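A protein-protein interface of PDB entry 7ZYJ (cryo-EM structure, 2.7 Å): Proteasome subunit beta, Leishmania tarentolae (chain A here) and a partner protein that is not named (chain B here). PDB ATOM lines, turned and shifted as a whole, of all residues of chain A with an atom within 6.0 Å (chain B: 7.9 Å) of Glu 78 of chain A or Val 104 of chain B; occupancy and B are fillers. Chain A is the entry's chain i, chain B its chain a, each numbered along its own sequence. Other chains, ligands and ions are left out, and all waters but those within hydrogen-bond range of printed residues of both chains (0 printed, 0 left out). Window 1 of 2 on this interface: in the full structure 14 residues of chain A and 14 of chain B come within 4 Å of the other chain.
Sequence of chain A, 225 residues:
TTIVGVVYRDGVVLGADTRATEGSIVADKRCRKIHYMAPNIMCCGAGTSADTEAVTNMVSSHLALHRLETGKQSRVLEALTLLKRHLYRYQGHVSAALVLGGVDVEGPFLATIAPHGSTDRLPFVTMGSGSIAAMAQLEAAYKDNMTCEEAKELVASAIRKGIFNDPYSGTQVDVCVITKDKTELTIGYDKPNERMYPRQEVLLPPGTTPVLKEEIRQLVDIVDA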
ATOM      1  N   VAL A  59      -6.488  22.248  25.500  1.00  0.00           N
ATOM      2  CA  VAL A  59      -5.201  22.739  25.974  1.00  0.00           C
ATOM      3  C   VAL A  59      -5.364  23.536  27.262  1.00  0.00           C
ATOM      4  O   VAL A  59      -4.504  23.471  28.146  1.00  0.00           O
ATOM      5  CB  VAL A  59      -4.494  23.550  24.872  1.00  0.00           C
ATOM      6  CG1 VAL A  59      -3.155  24.065  25.366  1.00  0.00           C
ATOM      7  CG2 VAL A  59      -4.281  22.677  23.652  1.00  0.00           C
ATOM      8  N   LEU A  63      -3.555  22.575  30.696  1.00  0.00           N
ATOM      9  CA  LEU A  63      -2.767  23.562  31.425  1.00  0.00           C
ATOM     10  C   LEU A  63      -3.235  23.693  32.867  1.00  0.00           C
ATOM     11  O   LEU A  63      -2.415  23.837  33.776  1.00  0.00           O
ATOM     12  CB  LEU A  63      -2.834  24.918  30.727  1.00  0.00           C
ATOM     13  CG  LEU A  63      -2.015  25.117  29.453  1.00  0.00           C
ATOM     14  CD1 LEU A  63      -2.080  26.571  29.036  1.00  0.00           C
ATOM     15  CD2 LEU A  63      -0.575  24.677  29.656  1.00  0.00           C
ATOM     16  N   HIS A  66      -1.875  20.879  34.687  1.00  0.00           N
ATOM     17  CA  HIS A  66      -0.439  21.050  34.865  1.00  0.00           C
ATOM     18  C   HIS A  66      -0.118  22.038  35.980  1.00  0.00           C
ATOM     19  O   HIS A  66       0.828  21.820  36.738  1.00  0.00           O
ATOM     20  CB  HIS A  66       0.199  21.497  33.552  1.00  0.00           C
ATOM     21  CG  HIS A  66       1.691  21.567  33.604  1.00  0.00           C
ATOM     22  ND1 HIS A  66       2.384  22.756  33.536  1.00  0.00           N
ATOM     23  CD2 HIS A  66       2.624  20.593  33.717  1.00  0.00           C
ATOM     24  CE1 HIS A  66       3.680  22.512  33.608  1.00  0.00           C
ATOM     25  NE2 HIS A  66       3.853  21.207  33.717  1.00  0.00           N
ATOM     26  N   GLN A  73       2.414  29.261  37.904  1.00  0.00           N
ATOM     27  CA  GLN A  73       1.565  29.773  36.842  1.00  0.00           C
ATOM     28  C   GLN A  73       2.050  29.247  35.498  1.00  0.00           C
ATOM     29  O   GLN A  73       3.241  28.988  35.299  1.00  0.00           O
ATOM     30  CB  GLN A  73       1.544  31.302  36.842  1.00  0.00           C
ATOM     31  CG  GLN A  73       2.745  31.955  36.188  1.00  0.00           C
ATOM     32  CD  GLN A  73       2.528  33.429  35.917  1.00  0.00           C
ATOM     33  OE1 GLN A  73       1.433  33.954  36.118  1.00  0.00           O
ATOM     34  NE2 GLN A  73       3.572  34.106  35.459  1.00  0.00           N
ATOM     35  N   SER A  74       1.110  29.066  34.578  1.00  0.00           N
ATOM     36  CA  SER A  74       1.426  28.472  33.289  1.00  0.00           C
ATOM     37  C   SER A  74       2.263  29.424  32.447  1.00  0.00           C
ATOM     38  O   SER A  74       2.070  30.642  32.477  1.00  0.00           O
ATOM     39  CB  SER A  74       0.145  28.102  32.543  1.00  0.00           C
ATOM     40  OG  SER A  74      -0.699  29.230  32.408  1.00  0.00           O
ATOM     41  N   ARG A  75       3.198  28.858  31.694  1.00  0.00           N
ATOM     42  CA  ARG A  75       4.032  29.617  30.779  1.00  0.00           C
ATOM     43  C   ARG A  75       3.392  29.622  29.399  1.00  0.00           C
ATOM     44  O   ARG A  75       2.787  28.631  28.981  1.00  0.00           O
ATOM     45  CB  ARG A  75       5.443  29.033  30.703  1.00  0.00           C
ATOM     46  CG  ARG A  75       6.165  28.983  32.037  1.00  0.00           C
ATOM     47  CD  ARG A  75       6.861  30.301  32.332  1.00  0.00           C
ATOM     48  NE  ARG A  75       7.652  30.247  33.556  1.00  0.00           N
ATOM     49  CZ  ARG A  75       8.834  29.655  33.664  1.00  0.00           C
ATOM     50  NH1 ARG A  75       9.405  29.059  32.630  1.00  0.00           N
ATOM     51  NH2 ARG A  75       9.459  29.664  34.837  1.00  0.00           N
ATOM     52  N   VAL A  76       3.522  30.748  28.696  1.00  0.00           N
ATOM     53  CA  VAL A  76       2.908  30.866  27.379  1.00  0.00           C
ATOM     54  C   VAL A  76       3.565  29.903  26.403  1.00  0.00           C
ATOM     55  O   VAL A  76       2.906  29.365  25.504  1.00  0.00           O
ATOM     56  CB  VAL A  76       2.987  32.325  26.889  1.00  0.00           C
ATOM     57  CG1 VAL A  76       2.439  32.444  25.481  1.00  0.00           C
ATOM     58  CG2 VAL A  76       2.247  33.241  27.841  1.00  0.00           C
ATOM     59  N   LEU A  77       4.868  29.660  26.568  1.00  0.00           N
ATOM     60  CA  LEU A  77       5.564  28.704  25.714  1.00  0.00           C
ATOM     61  C   LEU A  77       5.001  27.297  25.867  1.00  0.00           C
ATOM     62  O   LEU A  77       4.975  26.537  24.895  1.00  0.00           O
ATOM     63  CB  LEU A  77       7.059  28.716  26.031  1.00  0.00           C
ATOM     64  CG  LEU A  77       7.971  27.878  25.134  1.00  0.00           C
ATOM     65  CD1 LEU A  77       7.853  28.314  23.684  1.00  0.00           C
ATOM     66  CD2 LEU A  77       9.411  27.969  25.610  1.00  0.00           C
ATOM     67  N   GLU A  78       4.543  26.933  27.067  1.00  0.00           N
ATOM     68  CA  GLU A  78       3.944  25.616  27.259  1.00  0.00           C
ATOM     69  C   GLU A  78       2.651  25.474  26.464  1.00  0.00           C
ATOM     70  O   GLU A  78       2.435  24.458  25.788  1.00  0.00           O
ATOM     71  CB  GLU A  78       3.686  25.373  28.744  1.00  0.00           C
ATOM     72  CG  GLU A  78       4.947  25.239  29.573  1.00  0.00           C
ATOM     73  CD  GLU A  78       4.668  25.252  31.062  1.00  0.00           C
ATOM     74  OE1 GLU A  78       3.987  26.185  31.535  1.00  0.00           O
ATOM     75  OE2 GLU A  78       5.142  24.334  31.760  1.00  0.00           O
ATOM     76  N   ALA A  79       1.779  26.483  26.537  1.00  0.00           N
ATOM     77  CA  ALA A  79       0.551  26.463  25.752  1.00  0.00           C
ATOM     78  C   ALA A  79       0.858  26.445  24.262  1.00  0.00           C
ATOM     79  O   ALA A  79       0.203  25.732  23.492  1.00  0.00           O
ATOM     80  CB  ALA A  79      -0.318  27.669  26.104  1.00  0.00           C
ATOM     81  N   LEU A  80       1.853  27.229  23.841  1.00  0.00           N
ATOM     82  CA  LEU A  80       2.250  27.242  22.439  1.00  0.00           C
ATOM     83  C   LEU A  80       2.712  25.866  21.986  1.00  0.00           C
ATOM     84  O   LEU A  80       2.320  25.394  20.913  1.00  0.00           O
ATOM     85  CB  LEU A  80       3.355  28.275  22.222  1.00  0.00           C
ATOM     86  CG  LEU A  80       3.827  28.482  20.784  1.00  0.00           C
ATOM     87  CD1 LEU A  80       2.918  29.459  20.068  1.00  0.00           C
ATOM     88  CD2 LEU A  80       5.266  28.965  20.757  1.00  0.00           C
ATOM     89  N   THR A  81       3.538  25.201  22.797  1.00  0.00           N
ATOM     90  CA  THR A  81       4.029  23.877  22.438  1.00  0.00           C
ATOM     91  C   THR A  81       2.891  22.868  22.361  1.00  0.00           C
ATOM     92  O   THR A  81       2.825  22.075  21.417  1.00  0.00           O
ATOM     93  CB  THR A  81       5.082  23.416  23.444  1.00  0.00           C
ATOM     94  OG1 THR A  81       5.955  24.508  23.755  1.00  0.00           O
ATOM     95  CG2 THR A  81       5.898  22.272  22.867  1.00  0.00           C
ATOM     96  N   LEU A  82       1.980  22.889  23.338  1.00  0.00           N
ATOM     97  CA  LEU A  82       0.860  21.954  23.315  1.00  0.00           C
ATOM     98  C   LEU A  82      -0.001  22.163  22.074  1.00  0.00           C
ATOM     99  O   LEU A  82      -0.330  21.205  21.357  1.00  0.00           O
ATOM    100  CB  LEU A  82       0.023  22.106  24.584  1.00  0.00           C
ATOM    101  CG  LEU A  82       0.607  21.523  25.871  1.00  0.00           C
ATOM    102  CD1 LEU A  82      -0.180  22.004  27.075  1.00  0.00           C
ATOM    103  CD2 LEU A  82       0.622  20.005  25.813  1.00  0.00           C
ATOM    104  N   LEU A  83      -0.358  23.420  21.793  1.00  0.00           N
ATOM    105  CA  LEU A  83      -1.194  23.716  20.638  1.00  0.00           C
ATOM    106  C   LEU A  83      -0.506  23.321  19.339  1.00  0.00           C
ATOM    107  O   LEU A  83      -1.138  22.742  18.447  1.00  0.00           O
ATOM    108  CB  LEU A  83      -1.555  25.201  20.621  1.00  0.00           C
ATOM    109  CG  LEU A  83      -2.573  25.668  21.661  1.00  0.00           C
ATOM    110  CD1 LEU A  83      -2.452  27.163  21.899  1.00  0.00           C
ATOM    111  CD2 LEU A  83      -3.982  25.305  21.231  1.00  0.00           C
ATOM    112  N   ALA B  95      12.392  13.632  32.114  1.00  0.00           N
ATOM    113  CA  ALA B  95      12.760  14.984  31.720  1.00  0.00           C
ATOM    114  C   ALA B  95      12.559  15.178  30.223  1.00  0.00           C
ATOM    115  O   ALA B  95      11.822  16.076  29.796  1.00  0.00           O
ATOM    116  CB  ALA B  95      14.204  15.272  32.118  1.00  0.00           C
ATOM    117  N   SER B  96      13.163  14.302  29.416  1.00  0.00           N
ATOM    118  CA  SER B  96      13.176  14.492  27.969  1.00  0.00           C
ATOM    119  C   SER B  96      11.762  14.563  27.414  1.00  0.00           C
ATOM    120  O   SER B  96      11.399  15.521  26.720  1.00  0.00           O
ATOM    121  CB  SER B  96      13.963  13.362  27.302  1.00  0.00           C
ATOM    122  OG  SER B  96      15.223  13.185  27.921  1.00  0.00           O
ATOM    123  N   ASP B  97      10.935  13.566  27.742  1.00  0.00           N
ATOM    124  CA  ASP B  97       9.544  13.585  27.307  1.00  0.00           C
ATOM    125  C   ASP B  97       8.868  14.878  27.740  1.00  0.00           C
ATOM    126  O   ASP B  97       8.198  15.539  26.940  1.00  0.00           O
ATOM    127  CB  ASP B  97       8.800  12.371  27.865  1.00  0.00           C
ATOM    128  CG  ASP B  97       9.488  11.063  27.533  1.00  0.00           C
ATOM    129  OD1 ASP B  97      10.407  11.071  26.687  1.00  0.00           O
ATOM    130  OD2 ASP B  97       9.109  10.026  28.115  1.00  0.00           O
ATOM    131  N   TYR B  98       9.082  15.277  28.997  1.00  0.00           N
ATOM    132  CA  TYR B  98       8.525  16.538  29.471  1.00  0.00           C
ATOM    133  C   TYR B  98       8.991  17.686  28.589  1.00  0.00           C
ATOM    134  O   TYR B  98       8.179  18.491  28.115  1.00  0.00           O
ATOM    135  CB  TYR B  98       8.930  16.769  30.927  1.00  0.00           C
ATOM    136  CG  TYR B  98       8.230  17.928  31.602  1.00  0.00           C
ATOM    137  CD1 TYR B  98       8.649  19.235  31.394  1.00  0.00           C
ATOM    138  CD2 TYR B  98       7.160  17.713  32.458  1.00  0.00           C
ATOM    139  CE1 TYR B  98       8.017  20.292  32.009  1.00  0.00           C
ATOM    140  CE2 TYR B  98       6.522  18.767  33.078  1.00  0.00           C
ATOM    141  CZ  TYR B  98       6.956  20.054  32.850  1.00  0.00           C
ATOM    142  OH  TYR B  98       6.327  21.109  33.464  1.00  0.00           O
ATOM    143  N   GLN B  99      10.296  17.739  28.314  1.00  0.00           N
ATOM    144  CA  GLN B  99      10.830  18.790  27.456  1.00  0.00           C
ATOM    145  C   GLN B  99      10.171  18.759  26.086  1.00  0.00           C
ATOM    146  O   GLN B  99       9.914  19.809  25.486  1.00  0.00           O
ATOM    147  CB  GLN B  99      12.348  18.642  27.337  1.00  0.00           C
ATOM    148  CG  GLN B  99      12.965  19.402  26.176  1.00  0.00           C
ATOM    149  CD  GLN B  99      12.880  20.902  26.354  1.00  0.00           C
ATOM    150  OE1 GLN B  99      13.068  21.420  27.454  1.00  0.00           O
ATOM    151  NE2 GLN B  99      12.594  21.610  25.268  1.00  0.00           N
ATOM    152  N   TYR B 100       9.866  17.563  25.582  1.00  0.00           N
ATOM    153  CA  TYR B 100       9.256  17.468  24.266  1.00  0.00           C
ATOM    154  C   TYR B 100       7.761  17.750  24.293  1.00  0.00           C
ATOM    155  O   TYR B 100       7.181  18.029  23.240  1.00  0.00           O
ATOM    156  CB  TYR B 100       9.527  16.087  23.661  1.00  0.00           C
ATOM    157  CG  TYR B 100       9.029  15.929  22.242  1.00  0.00           C
ATOM    158  CD1 TYR B 100       9.798  16.353  21.168  1.00  0.00           C
ATOM    159  CD2 TYR B 100       7.800  15.338  21.975  1.00  0.00           C
ATOM    160  CE1 TYR B 100       9.353  16.211  19.870  1.00  0.00           C
ATOM    161  CE2 TYR B 100       7.347  15.192  20.680  1.00  0.00           C
ATOM    162  CZ  TYR B 100       8.128  15.628  19.632  1.00  0.00           C
ATOM    163  OH  TYR B 100       7.680  15.480  18.340  1.00  0.00           O
ATOM    164  N   ARG B 101       7.123  17.713  25.463  1.00  0.00           N
ATOM    165  CA  ARG B 101       5.680  17.915  25.493  1.00  0.00           C
ATOM    166  C   ARG B 101       5.288  19.332  25.879  1.00  0.00           C
ATOM    167  O   ARG B 101       4.212  19.796  25.483  1.00  0.00           O
ATOM    168  CB  ARG B 101       5.021  16.918  26.449  1.00  0.00           C
ATOM    169  CG  ARG B 101       5.150  15.470  26.002  1.00  0.00           C
ATOM    170  CD  ARG B 101       4.496  14.520  26.991  1.00  0.00           C
ATOM    171  NE  ARG B 101       3.050  14.697  27.032  1.00  0.00           N
ATOM    172  CZ  ARG B 101       2.387  15.226  28.051  1.00  0.00           C
ATOM    173  NH1 ARG B 101       3.011  15.642  29.141  1.00  0.00           N
ATOM    174  NH2 ARG B 101       1.065  15.341  27.974  1.00  0.00           N
ATOM    175  N   TYR B 102       6.130  20.033  26.635  1.00  0.00           N
ATOM    176  CA  TYR B 102       5.832  21.388  27.065  1.00  0.00           C
ATOM    177  C   TYR B 102       6.792  22.432  26.520  1.00  0.00           C
ATOM    178  O   TYR B 102       6.495  23.627  26.619  1.00  0.00           O
ATOM    179  CB  TYR B 102       5.823  21.469  28.598  1.00  0.00           C
ATOM    180  CG  TYR B 102       4.892  20.472  29.244  1.00  0.00           C
ATOM    181  CD1 TYR B 102       3.540  20.747  29.379  1.00  0.00           C
ATOM    182  CD2 TYR B 102       5.362  19.252  29.707  1.00  0.00           C
ATOM    183  CE1 TYR B 102       2.684  19.839  29.965  1.00  0.00           C
ATOM    184  CE2 TYR B 102       4.513  18.337  30.293  1.00  0.00           C
ATOM    185  CZ  TYR B 102       3.174  18.636  30.419  1.00  0.00           C
ATOM    186  OH  TYR B 102       2.321  17.728  31.003  1.00  0.00           O
ATOM    187  N   GLY B 103       7.927  22.027  25.953  1.00  0.00           N
ATOM    188  CA  GLY B 103       8.887  22.963  25.411  1.00  0.00           C
ATOM    189  C   GLY B 103       9.751  23.667  26.431  1.00  0.00           C
ATOM    190  O   GLY B 103      10.650  24.418  26.038  1.00  0.00           O
ATOM    191  N   VAL B 104       9.514  23.455  27.720  1.00  0.00           N
ATOM    192  CA  VAL B 104      10.323  24.046  28.773  1.00  0.00           C
ATOM    193  C   VAL B 104      10.986  22.924  29.558  1.00  0.00           C
ATOM    194  O   VAL B 104      10.545  21.772  29.549  1.00  0.00           O
ATOM    195  CB  VAL B 104       9.494  24.953  29.704  1.00  0.00           C
ATOM    196  CG1 VAL B 104       8.873  26.094  28.917  1.00  0.00           C
ATOM    197  CG2 VAL B 104       8.422  24.145  30.415  1.00  0.00           C
ATOM    198  N   GLU B 105      12.072  23.272  30.241  1.00  0.00           N
ATOM    199  CA  GLU B 105      12.773  22.303  31.066  1.00  0.00           C
ATOM    200  C   GLU B 105      11.932  21.941  32.285  1.00  0.00           C
ATOM    201  O   GLU B 105      11.229  22.782  32.854  1.00  0.00           O
ATOM    202  CB  GLU B 105      14.131  22.857  31.495  1.00  0.00           C
ATOM    203  CG  GLU B 105      14.979  21.886  32.295  1.00  0.00           C
ATOM    204  CD  GLU B 105      16.333  22.458  32.653  1.00  0.00           C
ATOM    205  OE1 GLU B 105      16.602  23.624  32.293  1.00  0.00           O
ATOM    206  OE2 GLU B 105      17.129  21.739  33.291  1.00  0.00           O
ATOM    207  N   ILE B 106      12.003  20.677  32.680  1.00  0.00           N
ATOM    208  CA  ILE B 106      11.144  20.175  33.760  1.00  0.00           C
ATOM    209  C   ILE B 106      11.562  20.807  35.082  1.00  0.00           C
ATOM    210  O   ILE B 106      12.770  20.927  35.357  1.00  0.00           O
ATOM    211  CB  ILE B 106      11.205  18.644  33.825  1.00  0.00           C
ATOM    212  CG1 ILE B 106      10.184  18.105  34.828  1.00  0.00           C
ATOM    213  CG2 ILE B 106      12.612  18.151  34.146  1.00  0.00           C
ATOM    214  CD1 ILE B 106       9.950  16.618  34.719  1.00  0.00           C
ATOM    215  N   PRO B 107      10.621  21.266  35.904  1.00  0.00           N
ATOM    216  CA  PRO B 107      10.980  21.727  37.248  1.00  0.00           C
ATOM    217  C   PRO B 107      11.446  20.573  38.121  1.00  0.00           C
ATOM    218  O   PRO B 107      11.060  19.419  37.926  1.00  0.00           O
ATOM    219  CB  PRO B 107       9.677  22.336  37.780  1.00  0.00           C
ATOM    220  CG  PRO B 107       8.835  22.580  36.568  1.00  0.00           C
ATOM    221  CD  PRO B 107       9.206  21.515  35.591  1.00  0.00           C
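The side-chain hydroxyl (OH) of Tyr 98 of chain B sits at hydrogen-bond distance from a ring nitrogen (NE2) of His 66 of chain A, at 2.5 Å. O of Tyr 102 of chain B lies within hydrogen-bond range of OG1 of Thr 81 of chain A (3.0 Å).
OE1 of Gln 99 of chain B lies close to O of Val 104 of chain B, 3.3 Å away. The side-chain hydroxyl of Tyr 102 of chain B lies within hydrogen-bond range of the guanidinium group of Arg 101 of chain B. The side-chain carboxylate of Glu 78 of chain A is in hydrogen-bond range of the backbone NH of Arg 75 of chain A, at 2.8 Å. The side-chain hydroxyl (OG1) of Thr 81 of chain A is in hydrogen-bond range of the backbone carbonyl oxygen (O) of Leu 77 of chain A, 2.5 Å away.
His 66 of chain A touches Tyr 102 of chain B. O of Tyr 102 of chain B touches O of Leu 77 of chain A, 3.7 Å away. CD2 of Leu 77 of chain A touches O of Gly 103 of chain B (3.8 Å). CD2 of Leu 77 of chain A touches CG1 of Val 104 of chain B, at 3.8 Å. OE2 of Glu 78 of chain A touches OH of Tyr 98 of chain B (3.8 Å). Glu 78 of chain A touches Tyr 102 of chain B (CA to O, 3.3 Å). Val 104 of chain B touches Glu 78 of chain A (CG2 to OE2, 3.6 Å). Thr 81 of chain A touches Arg 101 of chain B (CG2 to O, 3.98 Å). CG2 of Thr 81 of chain A touches N of Gly 103 of chain B, at 3.7 Å. Leu 82 of chain A touches Arg 101 of chain B.
Val 59 of chain A touches none of the printed residues of chain B. Of the printed residues of chain B, Leu 77 of chain A touches Tyr 102, Gly 103 and Val 104. Of the printed residues of chain B, Glu 78 of chain A touches Tyr 98 (3.8 Å), Tyr 102 (3.3 Å) and Val 104 (3.6 Å). No residue of chain B comes within 4 Å of Ala 79 of chain A. Printed residues of chain B within 4 Å of Leu 82 of chain A: Arg 101 (3.6 Å). Asp 97 of chain B touches none of the printed residues of chain A. Of the printed residues of chain A, Arg 101 of chain B touches Thr 81 and Leu 82. Of the printed residues of chain A, Tyr 102 of chain B touches His 66 (3.8 Å), Leu 77 (3.7 Å), Glu 78 (3.3 Å) and Thr 81 (3.0 Å). Of the printed residues of chain A, Gly 103 of chain B touches Leu 77 and Thr 81. Val 104 of chain B touches just these residues of chain A: Leu 77 and Glu 78. The nearest residue of chain B that does not touch Glu 78 of chain A is Arg 101 of chain B (5.0 Å). The nearest residue of chain A that does not touch Val 104 of chain B is Arg 75 of chain A (4.8 Å). The nearest printed residue of chain A that does not touch Arg 101 of chain B is Glu 78 of chain A (5.0 Å).
Hydrophobic or aromatic side chains of chain B that line the printed part of chain A: Tyr 98, Tyr 102 and Val 104. Of the 14 printed residues of chain A, 5 touch a printed residue of chain B. Hydrophobic or aromatic side chains of chain A within 4 Å of the printed part of chain B: His 66, Leu 77 and Leu 82. Among the printed residues, 12 pairs touch across the chains. Among the printed residues, no Asp or Glu carboxylate lies within 4 Å of a Lys or Arg side-chain nitrogen of the other chain.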
